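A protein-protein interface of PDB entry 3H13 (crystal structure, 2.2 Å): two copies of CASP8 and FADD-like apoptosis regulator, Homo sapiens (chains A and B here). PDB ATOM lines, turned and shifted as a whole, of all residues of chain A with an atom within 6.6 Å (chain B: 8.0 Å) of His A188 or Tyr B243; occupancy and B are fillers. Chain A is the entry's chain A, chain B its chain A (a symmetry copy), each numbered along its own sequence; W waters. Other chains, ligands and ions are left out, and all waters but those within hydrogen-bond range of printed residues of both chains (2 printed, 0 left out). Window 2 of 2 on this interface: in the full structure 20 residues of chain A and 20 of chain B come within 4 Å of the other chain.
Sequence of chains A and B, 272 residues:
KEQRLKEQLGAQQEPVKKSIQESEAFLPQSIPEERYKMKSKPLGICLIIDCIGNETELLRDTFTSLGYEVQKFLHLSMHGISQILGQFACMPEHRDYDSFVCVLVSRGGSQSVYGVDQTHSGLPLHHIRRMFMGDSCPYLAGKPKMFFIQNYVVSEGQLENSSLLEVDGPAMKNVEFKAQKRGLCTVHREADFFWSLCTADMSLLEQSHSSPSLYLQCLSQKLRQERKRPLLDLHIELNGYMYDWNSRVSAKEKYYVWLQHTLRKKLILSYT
The side-chain amide nitrogen (ND2) of Asn B239 sits at hydrogen-bond distance from the backbone carbonyl oxygen (O) of Leu A263.
Water W1 bridges O of Gly B240 (2.9 Å) and NH1 of Arg A264 (3.2 Å).
Water W2 lies within hydrogen-bond range of the backbone carbonyl oxygen (O) of His A261 (2.9 Å) and the side-chain amide nitrogen (ND2) of Asn B239 (3.2 Å).
Of the printed residues of chain B, His A188 touches Tyr B243.
Of chain A, only His A188, Glu A190, Ala A191, Thr A262 and Arg A264 come within 4 Å of Tyr B243.
Printed residues of chain B within 4 Å of Ala A191: Tyr B243.
Printed residues of chain B within 4 Å of Thr A262: Tyr B243.
Glu B237 touches none of the printed residues of chain A.
Lys B254 touches none of the printed residues of chain A.
The nearest residue of chain B that does not touch His A188 is Ser B247 (5.3 Å).
The nearest residue of chain A that does not touch Tyr B243 is Asp A192 (5.1 Å).
No position is printed for both chains.
His A188 touches Tyr B243 (CA to CE2, 3.7 Å).
Glu A190 touches Tyr B243 (O to OH, 3.7 Å).
Ala A191 touches Tyr B243 (CA to OH, 3.4 Å).
Ile B236 touches His A261.
CB of Thr A262 touches OH of Tyr B243, at 3.3 Å.
CD1 of Ile B236 touches O of Leu A263 (3.8 Å).
CG2 of Ile B236 touches C of Arg A264, 3.4 Å away.
Arg A264 touches Gly B240.
CD of Arg A264 touches CD1 of Tyr B243, 3.7 Å away.
Printed residues of chain A that touch a printed residue of chain B: His A188, Glu A190, Ala A191, His A261, Thr A262, Leu A263 and Arg A264.
Hydrophobic or aromatic side chains of chain A that line the printed part of chain B: Ala A191, His A261 and Leu A263.
Along chain A the printed residues that touch a printed residue of chain B span positions 188 to 264.
Of the 18 printed residues of chain B, 4 touch a printed residue of chain A.
Hydrophobic or aromatic side chains of chain B within 4 Å of the printed part of chain A: Ile B236 and Tyr B243.
The backbone carbonyl oxygen (O) of Glu A190 lies within hydrogen-bond range of the side-chain hydroxyl (OG1) of Thr A262, 2.5 Å away.
O of Thr A262 sits at hydrogen-bond distance from N of Asp A192, at 2.9 Å.
The side-chain carboxylate of Asp A192 lies within salt-bridge range of the guanidinium group of Arg A264, at 2.9 Å.
A ring nitrogen (ND1) of His A261 is in hydrogen-bond range of the backbone NH (N) of Leu A263.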
ATOM      1  N   GLY A 134     -19.923  13.684 -14.617  1.00  0.00           N
ATOM      2  CA  GLY A 134     -20.881  13.208 -13.632  1.00  0.00           C
ATOM      3  C   GLY A 134     -21.927  14.187 -13.131  1.00  0.00           C
ATOM      4  O   GLY A 134     -23.087  13.816 -12.952  1.00  0.00           O
ATOM      5  N   HIS A 188     -12.509  14.083  -9.890  1.00  0.00           N
ATOM      6  CA  HIS A 188     -13.488  13.023  -9.648  1.00  0.00           C
ATOM      7  C   HIS A 188     -14.590  12.985 -10.700  1.00  0.00           C
ATOM      8  O   HIS A 188     -14.887  11.928 -11.257  1.00  0.00           O
ATOM      9  CB  HIS A 188     -14.155  13.183  -8.281  1.00  0.00           C
ATOM     10  CG  HIS A 188     -15.397  12.358  -8.133  1.00  0.00           C
ATOM     11  ND1 HIS A 188     -15.365  10.988  -7.973  1.00  0.00           N
ATOM     12  CD2 HIS A 188     -16.706  12.695  -8.214  1.00  0.00           C
ATOM     13  CE1 HIS A 188     -16.600  10.518  -7.966  1.00  0.00           C
ATOM     14  NE2 HIS A 188     -17.432  11.534  -8.112  1.00  0.00           N
ATOM     15  N   ARG A 189     -15.219  14.136 -10.934  1.00  0.00           N
ATOM     16  CA  ARG A 189     -16.295  14.238 -11.916  1.00  0.00           C
ATOM     17  C   ARG A 189     -15.748  13.909 -13.300  1.00  0.00           C
ATOM     18  O   ARG A 189     -16.513  13.665 -14.237  1.00  0.00           O
ATOM     19  CB  ARG A 189     -16.872  15.657 -11.930  1.00  0.00           C
ATOM     20  CG  ARG A 189     -15.879  16.715 -12.391  1.00  0.00           C
ATOM     21  CD  ARG A 189     -16.529  18.089 -12.511  1.00  0.00           C
ATOM     22  NE  ARG A 189     -15.600  19.082 -13.053  1.00  0.00           N
ATOM     23  CZ  ARG A 189     -15.932  20.333 -13.366  1.00  0.00           C
ATOM     24  NH1 ARG A 189     -17.178  20.757 -13.194  1.00  0.00           N
ATOM     25  NH2 ARG A 189     -15.017  21.158 -13.861  1.00  0.00           N
ATOM     26  N   GLU A 190     -14.418  13.894 -13.406  1.00  0.00           N
ATOM     27  CA  GLU A 190     -13.739  13.617 -14.655  1.00  0.00           C
ATOM     28  C   GLU A 190     -13.191  12.200 -14.837  1.00  0.00           C
ATOM     29  O   GLU A 190     -12.446  11.955 -15.773  1.00  0.00           O
ATOM     30  CB  GLU A 190     -12.617  14.635 -14.874  1.00  0.00           C
ATOM     31  CG  GLU A 190     -11.530  14.609 -13.835  1.00  0.00           C
ATOM     32  CD  GLU A 190     -10.502  15.716 -14.052  1.00  0.00           C
ATOM     33  OE1 GLU A 190     -10.004  15.869 -15.199  1.00  0.00           O
ATOM     34  OE2 GLU A 190     -10.187  16.429 -13.070  1.00  0.00           O
ATOM     35  N   ALA A 191     -13.561  11.272 -13.958  1.00  0.00           N
ATOM     36  CA  ALA A 191     -13.106   9.882 -14.080  1.00  0.00           C
ATOM     37  C   ALA A 191     -13.910   9.165 -15.168  1.00  0.00           C
ATOM     38  O   ALA A 191     -14.983   9.622 -15.548  1.00  0.00           O
ATOM     39  CB  ALA A 191     -13.276   9.128 -12.733  1.00  0.00           C
ATOM     40  N   ASP A 192     -13.372   8.058 -15.679  1.00  0.00           N
ATOM     41  CA  ASP A 192     -14.058   7.241 -16.672  1.00  0.00           C
ATOM     42  C   ASP A 192     -14.243   7.838 -18.088  1.00  0.00           C
ATOM     43  O   ASP A 192     -15.143   7.412 -18.839  1.00  0.00           O
ATOM     44  CB  ASP A 192     -15.410   6.811 -16.097  1.00  0.00           C
ATOM     45  CG  ASP A 192     -15.296   6.314 -14.650  1.00  0.00           C
ATOM     46  OD1 ASP A 192     -16.044   6.828 -13.810  1.00  0.00           O
ATOM     47  OD2 ASP A 192     -14.464   5.425 -14.359  1.00  0.00           O
ATOM     48  N   HIS A 261      -6.872   9.860 -21.013  1.00  0.00           N
ATOM     49  CA  HIS A 261      -7.979   9.161 -20.372  1.00  0.00           C
ATOM     50  C   HIS A 261      -7.902   9.167 -18.839  1.00  0.00           C
ATOM     51  O   HIS A 261      -6.858   9.484 -18.241  1.00  0.00           O
ATOM     52  CB  HIS A 261      -8.111   7.729 -20.910  1.00  0.00           C
ATOM     53  CG  HIS A 261      -7.071   6.787 -20.401  1.00  0.00           C
ATOM     54  ND1 HIS A 261      -7.150   6.196 -19.157  1.00  0.00           N
ATOM     55  CD2 HIS A 261      -5.915   6.349 -20.955  1.00  0.00           C
ATOM     56  CE1 HIS A 261      -6.088   5.435 -18.966  1.00  0.00           C
ATOM     57  NE2 HIS A 261      -5.321   5.511 -20.040  1.00  0.00           N
ATOM     58  N   THR A 262      -9.031   8.857 -18.210  1.00  0.00           N
ATOM     59  CA  THR A 262      -9.117   8.788 -16.767  1.00  0.00           C
ATOM     60  C   THR A 262      -9.790   7.474 -16.367  1.00  0.00           C
ATOM     61  O   THR A 262     -10.544   7.413 -15.394  1.00  0.00           O
ATOM     62  CB  THR A 262      -9.897   9.990 -16.197  1.00  0.00           C
ATOM     63  OG1 THR A 262     -11.142  10.134 -16.894  1.00  0.00           O
ATOM     64  CG2 THR A 262      -9.067  11.278 -16.340  1.00  0.00           C
ATOM     65  N   LEU A 263      -9.504   6.416 -17.118  1.00  0.00           N
ATOM     66  CA  LEU A 263     -10.084   5.114 -16.828  1.00  0.00           C
ATOM     67  C   LEU A 263      -9.579   4.625 -15.484  1.00  0.00           C
ATOM     68  O   LEU A 263      -8.437   4.904 -15.107  1.00  0.00           O
ATOM     69  CB  LEU A 263      -9.712   4.103 -17.907  1.00  0.00           C
ATOM     70  CG  LEU A 263     -10.271   4.462 -19.284  1.00  0.00           C
ATOM     71  CD1 LEU A 263      -9.993   3.308 -20.261  1.00  0.00           C
ATOM     72  CD2 LEU A 263     -11.778   4.762 -19.152  1.00  0.00           C
ATOM     73  N   ARG A 264     -10.424   3.856 -14.794  1.00  0.00           N
ATOM     74  CA  ARG A 264     -10.106   3.345 -13.469  1.00  0.00           C
ATOM     75  C   ARG A 264     -10.137   1.841 -13.471  1.00  0.00           C
ATOM     76  O   ARG A 264      -9.823   1.222 -12.467  1.00  0.00           O
ATOM     77  CB  ARG A 264     -11.135   3.843 -12.436  1.00  0.00           C
ATOM     78  CG  ARG A 264     -11.199   5.343 -12.272  1.00  0.00           C
ATOM     79  CD  ARG A 264     -12.202   5.734 -11.174  1.00  0.00           C
ATOM     80  NE  ARG A 264     -13.581   5.549 -11.609  1.00  0.00           N
ATOM     81  CZ  ARG A 264     -14.407   4.602 -11.165  1.00  0.00           C
ATOM     82  NH1 ARG A 264     -14.003   3.730 -10.243  1.00  0.00           N
ATOM     83  NH2 ARG A 264     -15.637   4.507 -11.667  1.00  0.00           N
ATOM     84  N   ILE B 236      -3.551   2.134 -14.588  1.00  0.00           N
ATOM     85  CA  ILE B 236      -5.024   2.285 -14.552  1.00  0.00           C
ATOM     86  C   ILE B 236      -5.495   1.985 -13.120  1.00  0.00           C
ATOM     87  O   ILE B 236      -6.322   2.710 -12.559  1.00  0.00           O
ATOM     88  CB  ILE B 236      -5.744   1.274 -15.483  1.00  0.00           C
ATOM     89  CG1 ILE B 236      -5.515   1.629 -16.950  1.00  0.00           C
ATOM     90  CG2 ILE B 236      -7.248   1.218 -15.150  1.00  0.00           C
ATOM     91  CD1 ILE B 236      -6.000   2.965 -17.326  1.00  0.00           C
ATOM     92  N   GLU B 237      -4.970   0.904 -12.546  1.00  0.00           N
ATOM     93  CA  GLU B 237      -5.308   0.537 -11.166  1.00  0.00           C
ATOM     94  C   GLU B 237      -4.812   1.631 -10.230  1.00  0.00           C
ATOM     95  O   GLU B 237      -5.496   1.975  -9.270  1.00  0.00           O
ATOM     96  CB  GLU B 237      -4.676  -0.800 -10.799  1.00  0.00           C
ATOM     97  CG  GLU B 237      -5.011  -1.875 -11.822  1.00  0.00           C
ATOM     98  CD  GLU B 237      -4.624  -3.263 -11.364  1.00  0.00           C
ATOM     99  OE1 GLU B 237      -3.573  -3.418 -10.709  1.00  0.00           O
ATOM    100  OE2 GLU B 237      -5.383  -4.203 -11.670  1.00  0.00           O
ATOM    101  N   LEU B 238      -3.633   2.189 -10.502  1.00  0.00           N
ATOM    102  CA  LEU B 238      -3.148   3.282  -9.655  1.00  0.00           C
ATOM    103  C   LEU B 238      -4.140   4.459  -9.745  1.00  0.00           C
ATOM    104  O   LEU B 238      -4.434   5.077  -8.726  1.00  0.00           O
ATOM    105  CB  LEU B 238      -1.748   3.732 -10.078  1.00  0.00           C
ATOM    106  CG  LEU B 238      -1.089   4.871  -9.284  1.00  0.00           C
ATOM    107  CD1 LEU B 238       0.430   4.701  -9.321  1.00  0.00           C
ATOM    108  CD2 LEU B 238      -1.466   6.208  -9.873  1.00  0.00           C
ATOM    109  N   ASN B 239      -4.667   4.737 -10.949  1.00  0.00           N
ATOM    110  CA  ASN B 239      -5.658   5.823 -11.161  1.00  0.00           C
ATOM    111  C   ASN B 239      -6.836   5.579 -10.212  1.00  0.00           C
ATOM    112  O   ASN B 239      -7.242   6.465  -9.480  1.00  0.00           O
ATOM    113  CB  ASN B 239      -6.283   5.816 -12.574  1.00  0.00           C
ATOM    114  CG  ASN B 239      -5.395   6.405 -13.640  1.00  0.00           C
ATOM    115  OD1 ASN B 239      -4.344   6.993 -13.352  1.00  0.00           O
ATOM    116  ND2 ASN B 239      -5.836   6.266 -14.917  1.00  0.00           N
ATOM    117  N   GLY B 240      -7.377   4.362 -10.269  1.00  0.00           N
ATOM    118  CA  GLY B 240      -8.510   3.991  -9.438  1.00  0.00           C
ATOM    119  C   GLY B 240      -8.178   4.120  -7.958  1.00  0.00           C
ATOM    120  O   GLY B 240      -8.991   4.608  -7.182  1.00  0.00           O
ATOM    121  N   TYR B 241      -6.974   3.693  -7.579  1.00  0.00           N
ATOM    122  CA  TYR B 241      -6.508   3.786  -6.197  1.00  0.00           C
ATOM    123  C   TYR B 241      -6.458   5.259  -5.745  1.00  0.00           C
ATOM    124  O   TYR B 241      -6.943   5.595  -4.661  1.00  0.00           O
ATOM    125  CB  TYR B 241      -5.124   3.145  -6.096  1.00  0.00           C
ATOM    126  CG  TYR B 241      -4.542   3.060  -4.703  1.00  0.00           C
ATOM    127  CD1 TYR B 241      -4.609   1.874  -3.968  1.00  0.00           C
ATOM    128  CD2 TYR B 241      -3.886   4.148  -4.134  1.00  0.00           C
ATOM    129  CE1 TYR B 241      -4.023   1.778  -2.699  1.00  0.00           C
ATOM    130  CE2 TYR B 241      -3.304   4.063  -2.874  1.00  0.00           C
ATOM    131  CZ  TYR B 241      -3.372   2.875  -2.162  1.00  0.00           C
ATOM    132  OH  TYR B 241      -2.769   2.780  -0.924  1.00  0.00           O
ATOM    133  N   MET B 242      -5.897   6.146  -6.574  1.00  0.00           N
ATOM    134  CA  MET B 242      -5.821   7.575  -6.211  1.00  0.00           C
ATOM    135  C   MET B 242      -7.194   8.261  -6.165  1.00  0.00           C
ATOM    136  O   MET B 242      -7.409   9.165  -5.356  1.00  0.00           O
ATOM    137  CB  MET B 242      -4.926   8.355  -7.188  1.00  0.00           C
ATOM    138  CG  MET B 242      -3.444   8.001  -7.153  1.00  0.00           C
ATOM    139  SD  MET B 242      -2.711   8.138  -5.482  1.00  0.00           S
ATOM    140  CE  MET B 242      -2.181   6.646  -5.352  1.00  0.00           C
ATOM    141  N   TYR B 243      -8.106   7.865  -7.054  1.00  0.00           N
ATOM    142  CA  TYR B 243      -9.448   8.438  -7.073  1.00  0.00           C
ATOM    143  C   TYR B 243     -10.178   8.062  -5.781  1.00  0.00           C
ATOM    144  O   TYR B 243     -10.914   8.874  -5.221  1.00  0.00           O
ATOM    145  CB  TYR B 243     -10.282   7.906  -8.261  1.00  0.00           C
ATOM    146  CG  TYR B 243     -10.204   8.730  -9.534  1.00  0.00           C
ATOM    147  CD1 TYR B 243      -9.573   8.226 -10.684  1.00  0.00           C
ATOM    148  CD2 TYR B 243     -10.775  10.010  -9.601  1.00  0.00           C
ATOM    149  CE1 TYR B 243      -9.514   8.973 -11.875  1.00  0.00           C
ATOM    150  CE2 TYR B 243     -10.717  10.768 -10.770  1.00  0.00           C
ATOM    151  CZ  TYR B 243     -10.090  10.244 -11.908  1.00  0.00           C
ATOM    152  OH  TYR B 243     -10.064  10.984 -13.075  1.00  0.00           O
ATOM    153  N   ASP B 244      -9.993   6.819  -5.331  1.00  0.00           N
ATOM    154  CA  ASP B 244     -10.652   6.362  -4.116  1.00  0.00           C
ATOM    155  C   ASP B 244     -10.097   7.119  -2.907  1.00  0.00           C
ATOM    156  O   ASP B 244     -10.851   7.554  -2.036  1.00  0.00           O
ATOM    157  CB  ASP B 244     -10.473   4.857  -3.947  1.00  0.00           C
ATOM    158  CG  ASP B 244     -11.323   4.298  -2.816  1.00  0.00           C
ATOM    159  OD1 ASP B 244     -10.774   4.023  -1.730  1.00  0.00           O
ATOM    160  OD2 ASP B 244     -12.549   4.146  -3.007  1.00  0.00           O
ATOM    161  N   TRP B 245      -8.781   7.302  -2.866  1.00  0.00           N
ATOM    162  CA  TRP B 245      -8.171   8.045  -1.778  1.00  0.00           C
ATOM    163  C   TRP B 245      -8.714   9.476  -1.769  1.00  0.00           C
ATOM    164  O   TRP B 245      -9.143   9.984  -0.728  1.00  0.00           O
ATOM    165  CB  TRP B 245      -6.643   8.086  -1.933  1.00  0.00           C
ATOM    166  CG  TRP B 245      -5.983   9.188  -1.129  1.00  0.00           C
ATOM    167  CD1 TRP B 245      -5.574  10.401  -1.586  1.00  0.00           C
ATOM    168  CD2 TRP B 245      -5.634   9.143   0.265  1.00  0.00           C
ATOM    169  NE1 TRP B 245      -4.980  11.115  -0.571  1.00  0.00           N
ATOM    170  CE2 TRP B 245      -5.008  10.362   0.575  1.00  0.00           C
ATOM    171  CE3 TRP B 245      -5.796   8.181   1.279  1.00  0.00           C
ATOM    172  CZ2 TRP B 245      -4.535  10.659   1.866  1.00  0.00           C
ATOM    173  CZ3 TRP B 245      -5.332   8.472   2.560  1.00  0.00           C
ATOM    174  CH2 TRP B 245      -4.709   9.701   2.842  1.00  0.00           C
ATOM    175  N   ASN B 246      -8.707  10.110  -2.940  1.00  0.00           N
ATOM    176  CA  ASN B 246      -9.172  11.487  -3.063  1.00  0.00           C
ATOM    177  C   ASN B 246     -10.611  11.694  -2.606  1.00  0.00           C
ATOM    178  O   ASN B 246     -10.957  12.754  -2.074  1.00  0.00           O
ATOM    179  CB  ASN B 246      -9.055  11.957  -4.512  1.00  0.00           C
ATOM    180  CG  ASN B 246      -7.640  12.316  -4.898  1.00  0.00           C
ATOM    181  OD1 ASN B 246      -6.723  12.308  -4.064  1.00  0.00           O
ATOM    182  ND2 ASN B 246      -7.446  12.650  -6.176  1.00  0.00           N
ATOM    183  N   SER B 247     -11.450  10.687  -2.811  1.00  0.00           N
ATOM    184  CA  SER B 247     -12.843  10.820  -2.432  1.00  0.00           C
ATOM    185  C   SER B 247     -13.065  10.775  -0.915  1.00  0.00           C
ATOM    186  O   SER B 247     -14.136  11.136  -0.451  1.00  0.00           O
ATOM    187  CB  SER B 247     -13.678   9.724  -3.095  1.00  0.00           C
ATOM    188  OG  SER B 247     -13.400   8.477  -2.492  1.00  0.00           O
ATOM    189  N   ARG B 248     -12.061  10.349  -0.150  1.00  0.00           N
ATOM    190  CA  ARG B 248     -12.215  10.257   1.301  1.00  0.00           C
ATOM    191  C   ARG B 248     -11.480  11.318   2.108  1.00  0.00           C
ATOM    192  O   ARG B 248     -11.596  11.337   3.322  1.00  0.00           O
ATOM    193  CB  ARG B 248     -11.737   8.889   1.799  1.00  0.00           C
ATOM    194  CG  ARG B 248     -12.350   7.697   1.083  1.00  0.00           C
ATOM    195  CD  ARG B 248     -11.526   6.448   1.359  1.00  0.00           C
ATOM    196  NE  ARG B 248     -11.965   5.311   0.553  1.00  0.00           N
ATOM    197  CZ  ARG B 248     -13.121   4.675   0.718  1.00  0.00           C
ATOM    198  NH1 ARG B 248     -13.967   5.058   1.668  1.00  0.00           N
ATOM    199  NH2 ARG B 248     -13.434   3.650  -0.065  1.00  0.00           N
ATOM    200  N   VAL B 249     -10.731  12.203   1.463  1.00  0.00           N
ATOM    201  CA  VAL B 249      -9.970  13.182   2.231  1.00  0.00           C
ATOM    202  C   VAL B 249     -10.193  14.622   1.841  1.00  0.00           C
ATOM    203  O   VAL B 249     -10.868  14.909   0.857  1.00  0.00           O
ATOM    204  CB  VAL B 249      -8.464  12.864   2.133  1.00  0.00           C
ATOM    205  CG1 VAL B 249      -8.233  11.407   2.541  1.00  0.00           C
ATOM    206  CG2 VAL B 249      -7.961  13.112   0.717  1.00  0.00           C
ATOM    207  N   LYS B 254      -5.188  15.555  -1.299  1.00  0.00           N
ATOM    208  CA  LYS B 254      -5.396  14.850  -2.564  1.00  0.00           C
ATOM    209  C   LYS B 254      -4.189  14.744  -3.489  1.00  0.00           C
ATOM    210  O   LYS B 254      -3.248  15.515  -3.384  1.00  0.00           O
ATOM    211  CB  LYS B 254      -6.567  15.485  -3.326  1.00  0.00           C
ATOM    212  CG  LYS B 254      -7.882  15.291  -2.610  1.00  0.00           C
ATOM    213  CD  LYS B 254      -9.053  15.923  -3.333  1.00  0.00           C
ATOM    214  CE  LYS B 254     -10.335  15.750  -2.507  1.00  0.00           C
ATOM    215  NZ  LYS B 254     -11.526  16.341  -3.183  1.00  0.00           N
ATOM    216  N   TYR B 255      -4.235  13.770  -4.393  1.00  0.00           N
ATOM    217  CA  TYR B 255      -3.174  13.571  -5.369  1.00  0.00           C
ATOM    218  C   TYR B 255      -3.828  13.515  -6.725  1.00  0.00           C
ATOM    219  O   TYR B 255      -4.783  12.776  -6.921  1.00  0.00           O
ATOM    220  CB  TYR B 255      -2.412  12.260  -5.137  1.00  0.00           C
ATOM    221  CG  TYR B 255      -1.631  12.217  -3.848  1.00  0.00           C
ATOM    222  CD1 TYR B 255      -2.160  11.609  -2.710  1.00  0.00           C
ATOM    223  CD2 TYR B 255      -0.377  12.808  -3.752  1.00  0.00           C
ATOM    224  CE1 TYR B 255      -1.450  11.589  -1.504  1.00  0.00           C
ATOM    225  CE2 TYR B 255       0.338  12.805  -2.546  1.00  0.00           C
ATOM    226  CZ  TYR B 255      -0.205  12.191  -1.431  1.00  0.00           C
ATOM    227  OH  TYR B 255       0.491  12.188  -0.236  1.00  0.00           O
ATOM    228  N   TYR B 256      -3.313  14.310  -7.652  1.00  0.00           N
ATOM    229  CA  TYR B 256      -3.823  14.356  -9.008  1.00  0.00           C
ATOM    230  C   TYR B 256      -2.797  13.714  -9.939  1.00  0.00           C
ATOM    231  O   TYR B 256      -1.625  14.116  -9.971  1.00  0.00           O
ATOM    232  CB  TYR B 256      -4.079  15.809  -9.395  1.00  0.00           C
ATOM    233  CG  TYR B 256      -5.128  16.418  -8.502  1.00  0.00           C
ATOM    234  CD1 TYR B 256      -4.779  17.214  -7.409  1.00  0.00           C
ATOM    235  CD2 TYR B 256      -6.480  16.122  -8.701  1.00  0.00           C
ATOM    236  CE1 TYR B 256      -5.765  17.702  -6.532  1.00  0.00           C
ATOM    237  CE2 TYR B 256      -7.467  16.596  -7.833  1.00  0.00           C
ATOM    238  CZ  TYR B 256      -7.106  17.382  -6.761  1.00  0.00           C
ATOM    239  OH  TYR B 256      -8.096  17.867  -5.943  1.00  0.00           O
ATOM    240  N   VAL B 257      -3.235  12.716 -10.688  1.00  0.00           N
ATOM    241  CA  VAL B 257      -2.336  12.012 -11.580  1.00  0.00           C
ATOM    242  C   VAL B 257      -2.662  12.221 -13.038  1.00  0.00           C
ATOM    243  O   VAL B 257      -3.784  11.967 -13.477  1.00  0.00           O
ATOM    244  CB  VAL B 257      -2.342  10.500 -11.274  1.00  0.00           C
ATOM    245  CG1 VAL B 257      -1.283   9.784 -12.123  1.00  0.00           C
ATOM    246  CG2 VAL B 257      -2.056  10.286  -9.802  1.00  0.00           C
HETATM  247  O   HOH W   1     -11.723   4.384  -8.049  1.00  0.00           O
HETATM  248  O   HOH W   2      -4.559   8.023 -17.236  1.00  0.00           O
